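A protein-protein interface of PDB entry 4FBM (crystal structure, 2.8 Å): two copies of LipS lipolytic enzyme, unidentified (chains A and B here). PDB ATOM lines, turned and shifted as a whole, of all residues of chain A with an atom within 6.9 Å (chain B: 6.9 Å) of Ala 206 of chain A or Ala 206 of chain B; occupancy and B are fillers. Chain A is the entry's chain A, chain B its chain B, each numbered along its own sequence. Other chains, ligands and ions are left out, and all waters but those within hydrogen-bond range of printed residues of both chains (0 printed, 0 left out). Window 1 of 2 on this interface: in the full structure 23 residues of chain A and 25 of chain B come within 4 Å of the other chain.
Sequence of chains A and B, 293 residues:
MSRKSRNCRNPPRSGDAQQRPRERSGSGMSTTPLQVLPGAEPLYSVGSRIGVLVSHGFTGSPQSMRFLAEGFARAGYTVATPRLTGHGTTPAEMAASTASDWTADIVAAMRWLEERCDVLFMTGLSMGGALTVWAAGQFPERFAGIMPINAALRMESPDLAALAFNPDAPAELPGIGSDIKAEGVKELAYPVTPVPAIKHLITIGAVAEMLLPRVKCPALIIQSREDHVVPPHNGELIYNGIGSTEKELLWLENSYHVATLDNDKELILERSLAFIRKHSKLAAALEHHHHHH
The side-chain carboxylate (OE2) of Glu 209 of chain B lies within salt-bridge range of the guanidinium group (NH2) of Arg 154 of chain A (3.1 Å).
OG1 of Thr 203 of chain A lies within hydrogen-bond range of OG1 of Thr 203 of chain B (2.8 Å).
The side-chain carboxylate (OE2) of Glu 209 of chain A lies within salt-bridge range of the guanidinium group (NH2) of Arg 154 of chain B (2.8 Å).
NH2 of Arg 154 of chain B sits close to NH1 of Arg 154 of chain A, 3.4 Å away.
NH1 of Arg 154 of chain A is in salt-bridge range of OE1 of Glu 209 of chain A (2.8 Å).
The guanidinium group (NE) of Arg 154 of chain B lies within salt-bridge range of the side-chain carboxylate (OE1) of Glu 209 of chain B, at 3.0 Å.
Ala 161 of chain A touches Val 207 of chain B.
CB of Met 210 of chain B touches CB of Ala 161 of chain A, 3.9 Å away.
Leu 211 of chain B touches Ala 161 of chain A (CG to CB, 3.7 Å).
CG2 of Ile 202 of chain A touches CB of Ala 206 of chain B, 3.96 Å away.
Ile 202 of chain A touches Met 210 of chain B.
CB of Ala 206 of chain B touches CB of Ala 206 of chain A (3.7 Å).
Ala 161 of chain B touches Val 207 of chain A (O to CG1, 3.7 Å).
Ala 161 of chain B touches Met 210 of chain A.
Leu 211 of chain A touches Ala 161 of chain B (CD2 to CB, 3.7 Å).
Of chain B, only Ala 206 (3.7 Å) comes within 4 Å of Ala 206 of chain A.
Of chain A, only Ile 202 (3.96 Å) and Ala 206 (3.7 Å) come within 4 Å of Ala 206 of chain B.
No residue of chain B comes within 4 Å of Gly 205 of chain A.
No residue of chain A comes within 4 Å of Gly 205 of chain B.
Printed residues of chain B within 4 Å of Glu 209 of chain A: Arg 154.
Of the printed residues of chain B, Ala 161 of chain A touches Val 207 (3.9 Å), Met 210 (3.9 Å) and Leu 211 (3.7 Å).
Ala 130 of chain B touches none of the printed residues of chain A.
Hydrophobic or aromatic side chains of chain B that line the printed part of chain A: Ala 161, Ala 206, Val 207, Met 210 and Leu 211.
Of the 16 printed residues of chain A, 9 touch a printed residue of chain B.
Hydrophobic or aromatic side chains of chain A that line the printed part of chain B: Ala 161, Ile 202, Ala 206, Val 207, Met 210 and Leu 211.
Among the printed residues, Asp or Glu carboxylates within 4 Å of a Lys or Arg side-chain nitrogen of the other chain: Arg 154 of chain A with Glu 209 of chain B and Glu 209 of chain A with Arg 154 of chain B.
Arg 154 of chain A touches its own counterpart, Arg 154 of chain B.
Ala 161 of chain A touches Met 210 of chain B, and with the chains exchanged Met 210 of chain A touches Ala 161 of chain B.
Ala 161 of chain A touches Leu 211 of chain B, and with the chains exchanged Leu 211 of chain A touches Ala 161 of chain B.
Thr 203 of chain A touches its own counterpart, Thr 203 of chain B.
Of the 13 pairs that touch across the chains among the printed residues, 11 have their exchanged pair printed and touching as well.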
ATOM      1  N   ALA A 130      24.533  11.431  -4.845  1.00  0.00           N
ATOM      2  CA  ALA A 130      23.146  11.063  -4.803  1.00  0.00           C
ATOM      3  C   ALA A 130      22.812  10.366  -6.087  1.00  0.00           C
ATOM      4  O   ALA A 130      21.940   9.500  -6.117  1.00  0.00           O
ATOM      5  CB  ALA A 130      22.295  12.272  -4.609  1.00  0.00           C
ATOM      6  N   ALA A 152      24.520  14.160  -1.182  1.00  0.00           N
ATOM      7  CA  ALA A 152      23.562  15.252  -1.009  1.00  0.00           C
ATOM      8  C   ALA A 152      22.129  14.744  -1.097  1.00  0.00           C
ATOM      9  O   ALA A 152      21.446  15.049  -2.078  1.00  0.00           O
ATOM     10  CB  ALA A 152      23.803  16.314  -2.106  1.00  0.00           C
ATOM     11  N   LEU A 153      21.691  13.972  -0.097  1.00  0.00           N
ATOM     12  CA  LEU A 153      20.362  13.323  -0.109  1.00  0.00           C
ATOM     13  C   LEU A 153      19.288  14.160   0.548  1.00  0.00           C
ATOM     14  O   LEU A 153      18.152  14.198   0.071  1.00  0.00           O
ATOM     15  CB  LEU A 153      20.381  11.946   0.585  1.00  0.00           C
ATOM     16  CG  LEU A 153      20.379  10.694  -0.281  1.00  0.00           C
ATOM     17  CD1 LEU A 153      21.730  10.458  -0.857  1.00  0.00           C
ATOM     18  CD2 LEU A 153      19.989   9.482   0.507  1.00  0.00           C
ATOM     19  N   ARG A 154      19.637  14.771   1.680  1.00  0.00           N
ATOM     20  CA  ARG A 154      18.740  15.651   2.413  1.00  0.00           C
ATOM     21  C   ARG A 154      19.561  16.830   2.765  1.00  0.00           C
ATOM     22  O   ARG A 154      20.496  16.699   3.522  1.00  0.00           O
ATOM     23  CB  ARG A 154      18.290  14.996   3.678  1.00  0.00           C
ATOM     24  CG  ARG A 154      17.500  13.764   3.410  1.00  0.00           C
ATOM     25  CD  ARG A 154      17.104  13.099   4.703  1.00  0.00           C
ATOM     26  NE  ARG A 154      16.193  13.945   5.452  1.00  0.00           N
ATOM     27  CZ  ARG A 154      14.909  14.075   5.163  1.00  0.00           C
ATOM     28  NH1 ARG A 154      14.379  13.406   4.134  1.00  0.00           N
ATOM     29  NH2 ARG A 154      14.157  14.881   5.907  1.00  0.00           N
ATOM     30  N   ALA A 161      14.941  25.496   0.204  1.00  0.00           N
ATOM     31  CA  ALA A 161      13.654  24.992  -0.233  1.00  0.00           C
ATOM     32  C   ALA A 161      12.760  26.149  -0.616  1.00  0.00           C
ATOM     33  O   ALA A 161      11.995  26.069  -1.554  1.00  0.00           O
ATOM     34  CB  ALA A 161      13.009  24.157   0.862  1.00  0.00           C
ATOM     35  N   LEU A 201      18.231  19.814  -7.839  1.00  0.00           N
ATOM     36  CA  LEU A 201      19.097  19.284  -6.793  1.00  0.00           C
ATOM     37  C   LEU A 201      18.309  18.512  -5.688  1.00  0.00           C
ATOM     38  O   LEU A 201      18.713  17.407  -5.277  1.00  0.00           O
ATOM     39  CB  LEU A 201      19.989  20.374  -6.180  1.00  0.00           C
ATOM     40  CG  LEU A 201      20.547  19.935  -4.811  1.00  0.00           C
ATOM     41  CD1 LEU A 201      21.631  18.828  -4.908  1.00  0.00           C
ATOM     42  CD2 LEU A 201      21.063  21.098  -4.032  1.00  0.00           C
ATOM     43  N   ILE A 202      17.197  19.085  -5.227  1.00  0.00           N
ATOM     44  CA  ILE A 202      16.380  18.449  -4.203  1.00  0.00           C
ATOM     45  C   ILE A 202      15.718  17.185  -4.712  1.00  0.00           C
ATOM     46  O   ILE A 202      15.635  16.185  -3.984  1.00  0.00           O
ATOM     47  CB  ILE A 202      15.335  19.425  -3.668  1.00  0.00           C
ATOM     48  CG1 ILE A 202      16.067  20.616  -3.051  1.00  0.00           C
ATOM     49  CG2 ILE A 202      14.419  18.750  -2.641  1.00  0.00           C
ATOM     50  CD1 ILE A 202      15.247  21.870  -2.911  1.00  0.00           C
ATOM     51  N   THR A 203      15.255  17.231  -5.963  1.00  0.00           N
ATOM     52  CA  THR A 203      14.598  16.070  -6.579  1.00  0.00           C
ATOM     53  C   THR A 203      15.518  14.875  -6.557  1.00  0.00           C
ATOM     54  O   THR A 203      15.156  13.826  -6.062  1.00  0.00           O
ATOM     55  CB  THR A 203      14.221  16.308  -8.025  1.00  0.00           C
ATOM     56  OG1 THR A 203      13.399  17.472  -8.107  1.00  0.00           O
ATOM     57  CG2 THR A 203      13.454  15.124  -8.554  1.00  0.00           C
ATOM     58  N   ILE A 204      16.710  15.050  -7.105  1.00  0.00           N
ATOM     59  CA  ILE A 204      17.721  13.999  -7.108  1.00  0.00           C
ATOM     60  C   ILE A 204      17.916  13.413  -5.705  1.00  0.00           C
ATOM     61  O   ILE A 204      17.954  12.189  -5.537  1.00  0.00           O
ATOM     62  CB  ILE A 204      19.081  14.550  -7.576  1.00  0.00           C
ATOM     63  CG1 ILE A 204      19.077  14.811  -9.075  1.00  0.00           C
ATOM     64  CG2 ILE A 204      20.191  13.599  -7.207  1.00  0.00           C
ATOM     65  CD1 ILE A 204      18.986  13.533  -9.853  1.00  0.00           C
ATOM     66  N   GLY A 205      18.047  14.307  -4.717  1.00  0.00           N
ATOM     67  CA  GLY A 205      18.306  13.922  -3.342  1.00  0.00           C
ATOM     68  C   GLY A 205      17.191  13.064  -2.795  1.00  0.00           C
ATOM     69  O   GLY A 205      17.432  12.076  -2.103  1.00  0.00           O
ATOM     70  N   ALA A 206      15.964  13.441  -3.124  1.00  0.00           N
ATOM     71  CA  ALA A 206      14.789  12.780  -2.606  1.00  0.00           C
ATOM     72  C   ALA A 206      14.524  11.446  -3.292  1.00  0.00           C
ATOM     73  O   ALA A 206      14.111  10.489  -2.617  1.00  0.00           O
ATOM     74  CB  ALA A 206      13.603  13.684  -2.731  1.00  0.00           C
ATOM     75  N   VAL A 207      14.735  11.373  -4.613  1.00  0.00           N
ATOM     76  CA  VAL A 207      14.583  10.110  -5.351  1.00  0.00           C
ATOM     77  C   VAL A 207      15.586   9.072  -4.834  1.00  0.00           C
ATOM     78  O   VAL A 207      15.203   7.963  -4.458  1.00  0.00           O
ATOM     79  CB  VAL A 207      14.651  10.293  -6.898  1.00  0.00           C
ATOM     80  CG1 VAL A 207      14.720   8.966  -7.606  1.00  0.00           C
ATOM     81  CG2 VAL A 207      13.415  10.960  -7.360  1.00  0.00           C
ATOM     82  N   ALA A 208      16.857   9.457  -4.780  1.00  0.00           N
ATOM     83  CA  ALA A 208      17.896   8.623  -4.178  1.00  0.00           C
ATOM     84  C   ALA A 208      17.459   8.097  -2.829  1.00  0.00           C
ATOM     85  O   ALA A 208      17.586   6.895  -2.573  1.00  0.00           O
ATOM     86  CB  ALA A 208      19.207   9.378  -4.041  1.00  0.00           C
ATOM     87  N   GLU A 209      16.947   8.984  -1.970  1.00  0.00           N
ATOM     88  CA  GLU A 209      16.558   8.569  -0.619  1.00  0.00           C
ATOM     89  C   GLU A 209      15.531   7.447  -0.649  1.00  0.00           C
ATOM     90  O   GLU A 209      15.663   6.449   0.072  1.00  0.00           O
ATOM     91  CB  GLU A 209      16.026   9.718   0.237  1.00  0.00           C
ATOM     92  CG  GLU A 209      15.809   9.286   1.699  1.00  0.00           C
ATOM     93  CD  GLU A 209      15.294  10.400   2.606  1.00  0.00           C
ATOM     94  OE1 GLU A 209      15.055  11.550   2.125  1.00  0.00           O
ATOM     95  OE2 GLU A 209      15.122  10.125   3.821  1.00  0.00           O
ATOM     96  N   MET A 210      14.528   7.632  -1.499  1.00  0.00           N
ATOM     97  CA  MET A 210      13.409   6.735  -1.587  1.00  0.00           C
ATOM     98  C   MET A 210      13.855   5.385  -2.195  1.00  0.00           C
ATOM     99  O   MET A 210      13.242   4.343  -1.913  1.00  0.00           O
ATOM    100  CB  MET A 210      12.297   7.419  -2.386  1.00  0.00           C
ATOM    101  CG  MET A 210      10.905   6.958  -2.028  1.00  0.00           C
ATOM    102  SD  MET A 210       9.619   7.656  -3.126  1.00  0.00           S
ATOM    103  CE  MET A 210       9.132   9.131  -2.216  1.00  0.00           C
ATOM    104  N   LEU A 211      14.935   5.406  -2.985  1.00  0.00           N
ATOM    105  CA  LEU A 211      15.531   4.198  -3.568  1.00  0.00           C
ATOM    106  C   LEU A 211      16.475   3.390  -2.667  1.00  0.00           C
ATOM    107  O   LEU A 211      16.881   2.318  -3.064  1.00  0.00           O
ATOM    108  CB  LEU A 211      16.273   4.536  -4.863  1.00  0.00           C
ATOM    109  CG  LEU A 211      15.501   4.914  -6.129  1.00  0.00           C
ATOM    110  CD1 LEU A 211      16.449   5.386  -7.196  1.00  0.00           C
ATOM    111  CD2 LEU A 211      14.651   3.784  -6.667  1.00  0.00           C
ATOM    112  N   ALA B 130       0.428  18.507   0.270  1.00  0.00           N
ATOM    113  CA  ALA B 130       1.839  18.836   0.248  1.00  0.00           C
ATOM    114  C   ALA B 130       1.966  20.278  -0.231  1.00  0.00           C
ATOM    115  O   ALA B 130       2.790  21.055   0.286  1.00  0.00           O
ATOM    116  CB  ALA B 130       2.581  17.887  -0.638  1.00  0.00           C
ATOM    117  N   ALA B 152       0.854  14.363   0.858  1.00  0.00           N
ATOM    118  CA  ALA B 152       1.825  13.489   0.174  1.00  0.00           C
ATOM    119  C   ALA B 152       3.292  13.947   0.278  1.00  0.00           C
ATOM    120  O   ALA B 152       3.956  14.232  -0.732  1.00  0.00           O
ATOM    121  CB  ALA B 152       1.412  13.298  -1.280  1.00  0.00           C
ATOM    122  N   LEU B 153       3.784  14.025   1.498  1.00  0.00           N
ATOM    123  CA  LEU B 153       5.156  14.444   1.744  1.00  0.00           C
ATOM    124  C   LEU B 153       6.212  13.426   1.431  1.00  0.00           C
ATOM    125  O   LEU B 153       7.241  13.762   0.872  1.00  0.00           O
ATOM    126  CB  LEU B 153       5.330  14.948   3.187  1.00  0.00           C
ATOM    127  CG  LEU B 153       5.324  16.472   3.357  1.00  0.00           C
ATOM    128  CD1 LEU B 153       3.981  17.091   3.031  1.00  0.00           C
ATOM    129  CD2 LEU B 153       5.750  16.842   4.723  1.00  0.00           C
ATOM    130  N   ARG B 154       5.978  12.189   1.844  1.00  0.00           N
ATOM    131  CA  ARG B 154       6.898  11.100   1.601  1.00  0.00           C
ATOM    132  C   ARG B 154       6.130   9.932   1.148  1.00  0.00           C
ATOM    133  O   ARG B 154       5.452   9.329   1.935  1.00  0.00           O
ATOM    134  CB  ARG B 154       7.549  10.700   2.882  1.00  0.00           C
ATOM    135  CG  ARG B 154       8.153  11.832   3.527  1.00  0.00           C
ATOM    136  CD  ARG B 154       8.899  11.378   4.686  1.00  0.00           C
ATOM    137  NE  ARG B 154      10.309  11.459   4.383  1.00  0.00           N
ATOM    138  CZ  ARG B 154      11.151  10.454   4.497  1.00  0.00           C
ATOM    139  NH1 ARG B 154      10.719   9.285   4.938  1.00  0.00           N
ATOM    140  NH2 ARG B 154      12.416  10.645   4.183  1.00  0.00           N
ATOM    141  N   ALA B 161       9.876   5.600  -7.039  1.00  0.00           N
ATOM    142  CA  ALA B 161      11.117   6.290  -7.303  1.00  0.00           C
ATOM    143  C   ALA B 161      11.858   5.678  -8.485  1.00  0.00           C
ATOM    144  O   ALA B 161      12.548   6.372  -9.222  1.00  0.00           O
ATOM    145  CB  ALA B 161      11.972   6.261  -6.086  1.00  0.00           C
ATOM    146  N   LEU B 201       5.655  15.013  -8.455  1.00  0.00           N
ATOM    147  CA  LEU B 201       4.988  14.653  -7.214  1.00  0.00           C
ATOM    148  C   LEU B 201       6.004  14.498  -6.081  1.00  0.00           C
ATOM    149  O   LEU B 201       5.736  14.885  -4.956  1.00  0.00           O
ATOM    150  CB  LEU B 201       4.222  13.350  -7.419  1.00  0.00           C
ATOM    151  CG  LEU B 201       3.741  12.529  -6.236  1.00  0.00           C
ATOM    152  CD1 LEU B 201       2.843  13.368  -5.362  1.00  0.00           C
ATOM    153  CD2 LEU B 201       2.993  11.357  -6.786  1.00  0.00           C
ATOM    154  N   ILE B 202       7.164  13.931  -6.395  1.00  0.00           N
ATOM    155  CA  ILE B 202       8.167  13.632  -5.391  1.00  0.00           C
ATOM    156  C   ILE B 202       8.817  14.938  -4.934  1.00  0.00           C
ATOM    157  O   ILE B 202       9.100  15.125  -3.756  1.00  0.00           O
ATOM    158  CB  ILE B 202       9.208  12.623  -5.947  1.00  0.00           C
ATOM    159  CG1 ILE B 202       8.537  11.272  -6.221  1.00  0.00           C
ATOM    160  CG2 ILE B 202      10.379  12.427  -4.994  1.00  0.00           C
ATOM    161  CD1 ILE B 202       9.417  10.263  -6.913  1.00  0.00           C
ATOM    162  N   THR B 203       9.021  15.843  -5.877  1.00  0.00           N
ATOM    163  CA  THR B 203       9.709  17.086  -5.608  1.00  0.00           C
ATOM    164  C   THR B 203       8.857  17.935  -4.655  1.00  0.00           C
ATOM    165  O   THR B 203       9.364  18.476  -3.681  1.00  0.00           O
ATOM    166  CB  THR B 203       9.995  17.834  -6.937  1.00  0.00           C
ATOM    167  OG1 THR B 203      10.672  16.939  -7.828  1.00  0.00           O
ATOM    168  CG2 THR B 203      10.846  19.036  -6.736  1.00  0.00           C
ATOM    169  N   ILE B 204       7.561  18.042  -4.928  1.00  0.00           N
ATOM    170  CA  ILE B 204       6.682  18.843  -4.073  1.00  0.00           C
ATOM    171  C   ILE B 204       6.671  18.268  -2.646  1.00  0.00           C
ATOM    172  O   ILE B 204       6.781  19.012  -1.656  1.00  0.00           O
ATOM    173  CB  ILE B 204       5.265  18.913  -4.657  1.00  0.00           C
ATOM    174  CG1 ILE B 204       5.250  19.839  -5.858  1.00  0.00           C
ATOM    175  CG2 ILE B 204       4.270  19.409  -3.642  1.00  0.00           C
ATOM    176  CD1 ILE B 204       4.305  19.415  -6.935  1.00  0.00           C
ATOM    177  N   GLY B 205       6.566  16.946  -2.539  1.00  0.00           N
ATOM    178  CA  GLY B 205       6.665  16.292  -1.236  1.00  0.00           C
ATOM    179  C   GLY B 205       7.964  16.606  -0.490  1.00  0.00           C
ATOM    180  O   GLY B 205       7.960  16.782   0.724  1.00  0.00           O
ATOM    181  N   ALA B 206       9.070  16.682  -1.214  1.00  0.00           N
ATOM    182  CA  ALA B 206      10.358  16.794  -0.590  1.00  0.00           C
ATOM    183  C   ALA B 206      10.569  18.224  -0.140  1.00  0.00           C
ATOM    184  O   ALA B 206      11.049  18.473   0.990  1.00  0.00           O
ATOM    185  CB  ALA B 206      11.432  16.385  -1.562  1.00  0.00           C
ATOM    186  N   VAL B 207      10.212  19.152  -1.040  1.00  0.00           N
ATOM    187  CA  VAL B 207      10.341  20.592  -0.843  1.00  0.00           C
ATOM    188  C   VAL B 207       9.456  20.958   0.338  1.00  0.00           C
ATOM    189  O   VAL B 207       9.880  21.683   1.255  1.00  0.00           O
ATOM    190  CB  VAL B 207       9.953  21.393  -2.148  1.00  0.00           C
ATOM    191  CG1 VAL B 207       9.766  22.853  -1.875  1.00  0.00           C
ATOM    192  CG2 VAL B 207      11.018  21.245  -3.189  1.00  0.00           C
ATOM    193  N   ALA B 208       8.238  20.413   0.330  1.00  0.00           N
ATOM    194  CA  ALA B 208       7.303  20.679   1.401  1.00  0.00           C
ATOM    195  C   ALA B 208       7.876  20.238   2.728  1.00  0.00           C
ATOM    196  O   ALA B 208       7.772  20.986   3.703  1.00  0.00           O
ATOM    197  CB  ALA B 208       5.986  20.013   1.154  1.00  0.00           C
ATOM    198  N   GLU B 209       8.481  19.048   2.774  1.00  0.00           N
ATOM    199  CA  GLU B 209       8.995  18.523   4.027  1.00  0.00           C
ATOM    200  C   GLU B 209      10.152  19.380   4.502  1.00  0.00           C
ATOM    201  O   GLU B 209      10.293  19.636   5.698  1.00  0.00           O
ATOM    202  CB  GLU B 209       9.410  17.068   3.906  1.00  0.00           C
ATOM    203  CG  GLU B 209      10.526  16.693   4.863  1.00  0.00           C
ATOM    204  CD  GLU B 209      10.685  15.187   5.087  1.00  0.00           C
ATOM    205  OE1 GLU B 209      10.402  14.402   4.149  1.00  0.00           O
ATOM    206  OE2 GLU B 209      11.116  14.781   6.199  1.00  0.00           O
ATOM    207  N   MET B 210      10.966  19.863   3.571  1.00  0.00           N
ATOM    208  CA  MET B 210      12.125  20.662   3.957  1.00  0.00           C
ATOM    209  C   MET B 210      11.764  22.051   4.523  1.00  0.00           C
ATOM    210  O   MET B 210      12.569  22.675   5.214  1.00  0.00           O
ATOM    211  CB  MET B 210      13.085  20.794   2.779  1.00  0.00           C
ATOM    212  CG  MET B 210      14.527  20.995   3.212  1.00  0.00           C
ATOM    213  SD  MET B 210      15.710  21.341   1.880  1.00  0.00           S
ATOM    214  CE  MET B 210      15.300  19.985   0.783  1.00  0.00           C
ATOM    215  N   LEU B 211      10.563  22.523   4.210  1.00  0.00           N
ATOM    216  CA  LEU B 211      10.073  23.816   4.647  1.00  0.00           C
ATOM    217  C   LEU B 211       9.282  23.728   5.961  1.00  0.00           C
ATOM    218  O   LEU B 211       8.872  24.772   6.492  1.00  0.00           O
ATOM    219  CB  LEU B 211       9.157  24.417   3.591  1.00  0.00           C
ATOM    220  CG  LEU B 211       9.781  25.111   2.410  1.00  0.00           C
ATOM    221  CD1 LEU B 211       8.815  25.093   1.260  1.00  0.00           C
ATOM    222  CD2 LEU B 211      10.177  26.533   2.747  1.00  0.00           C
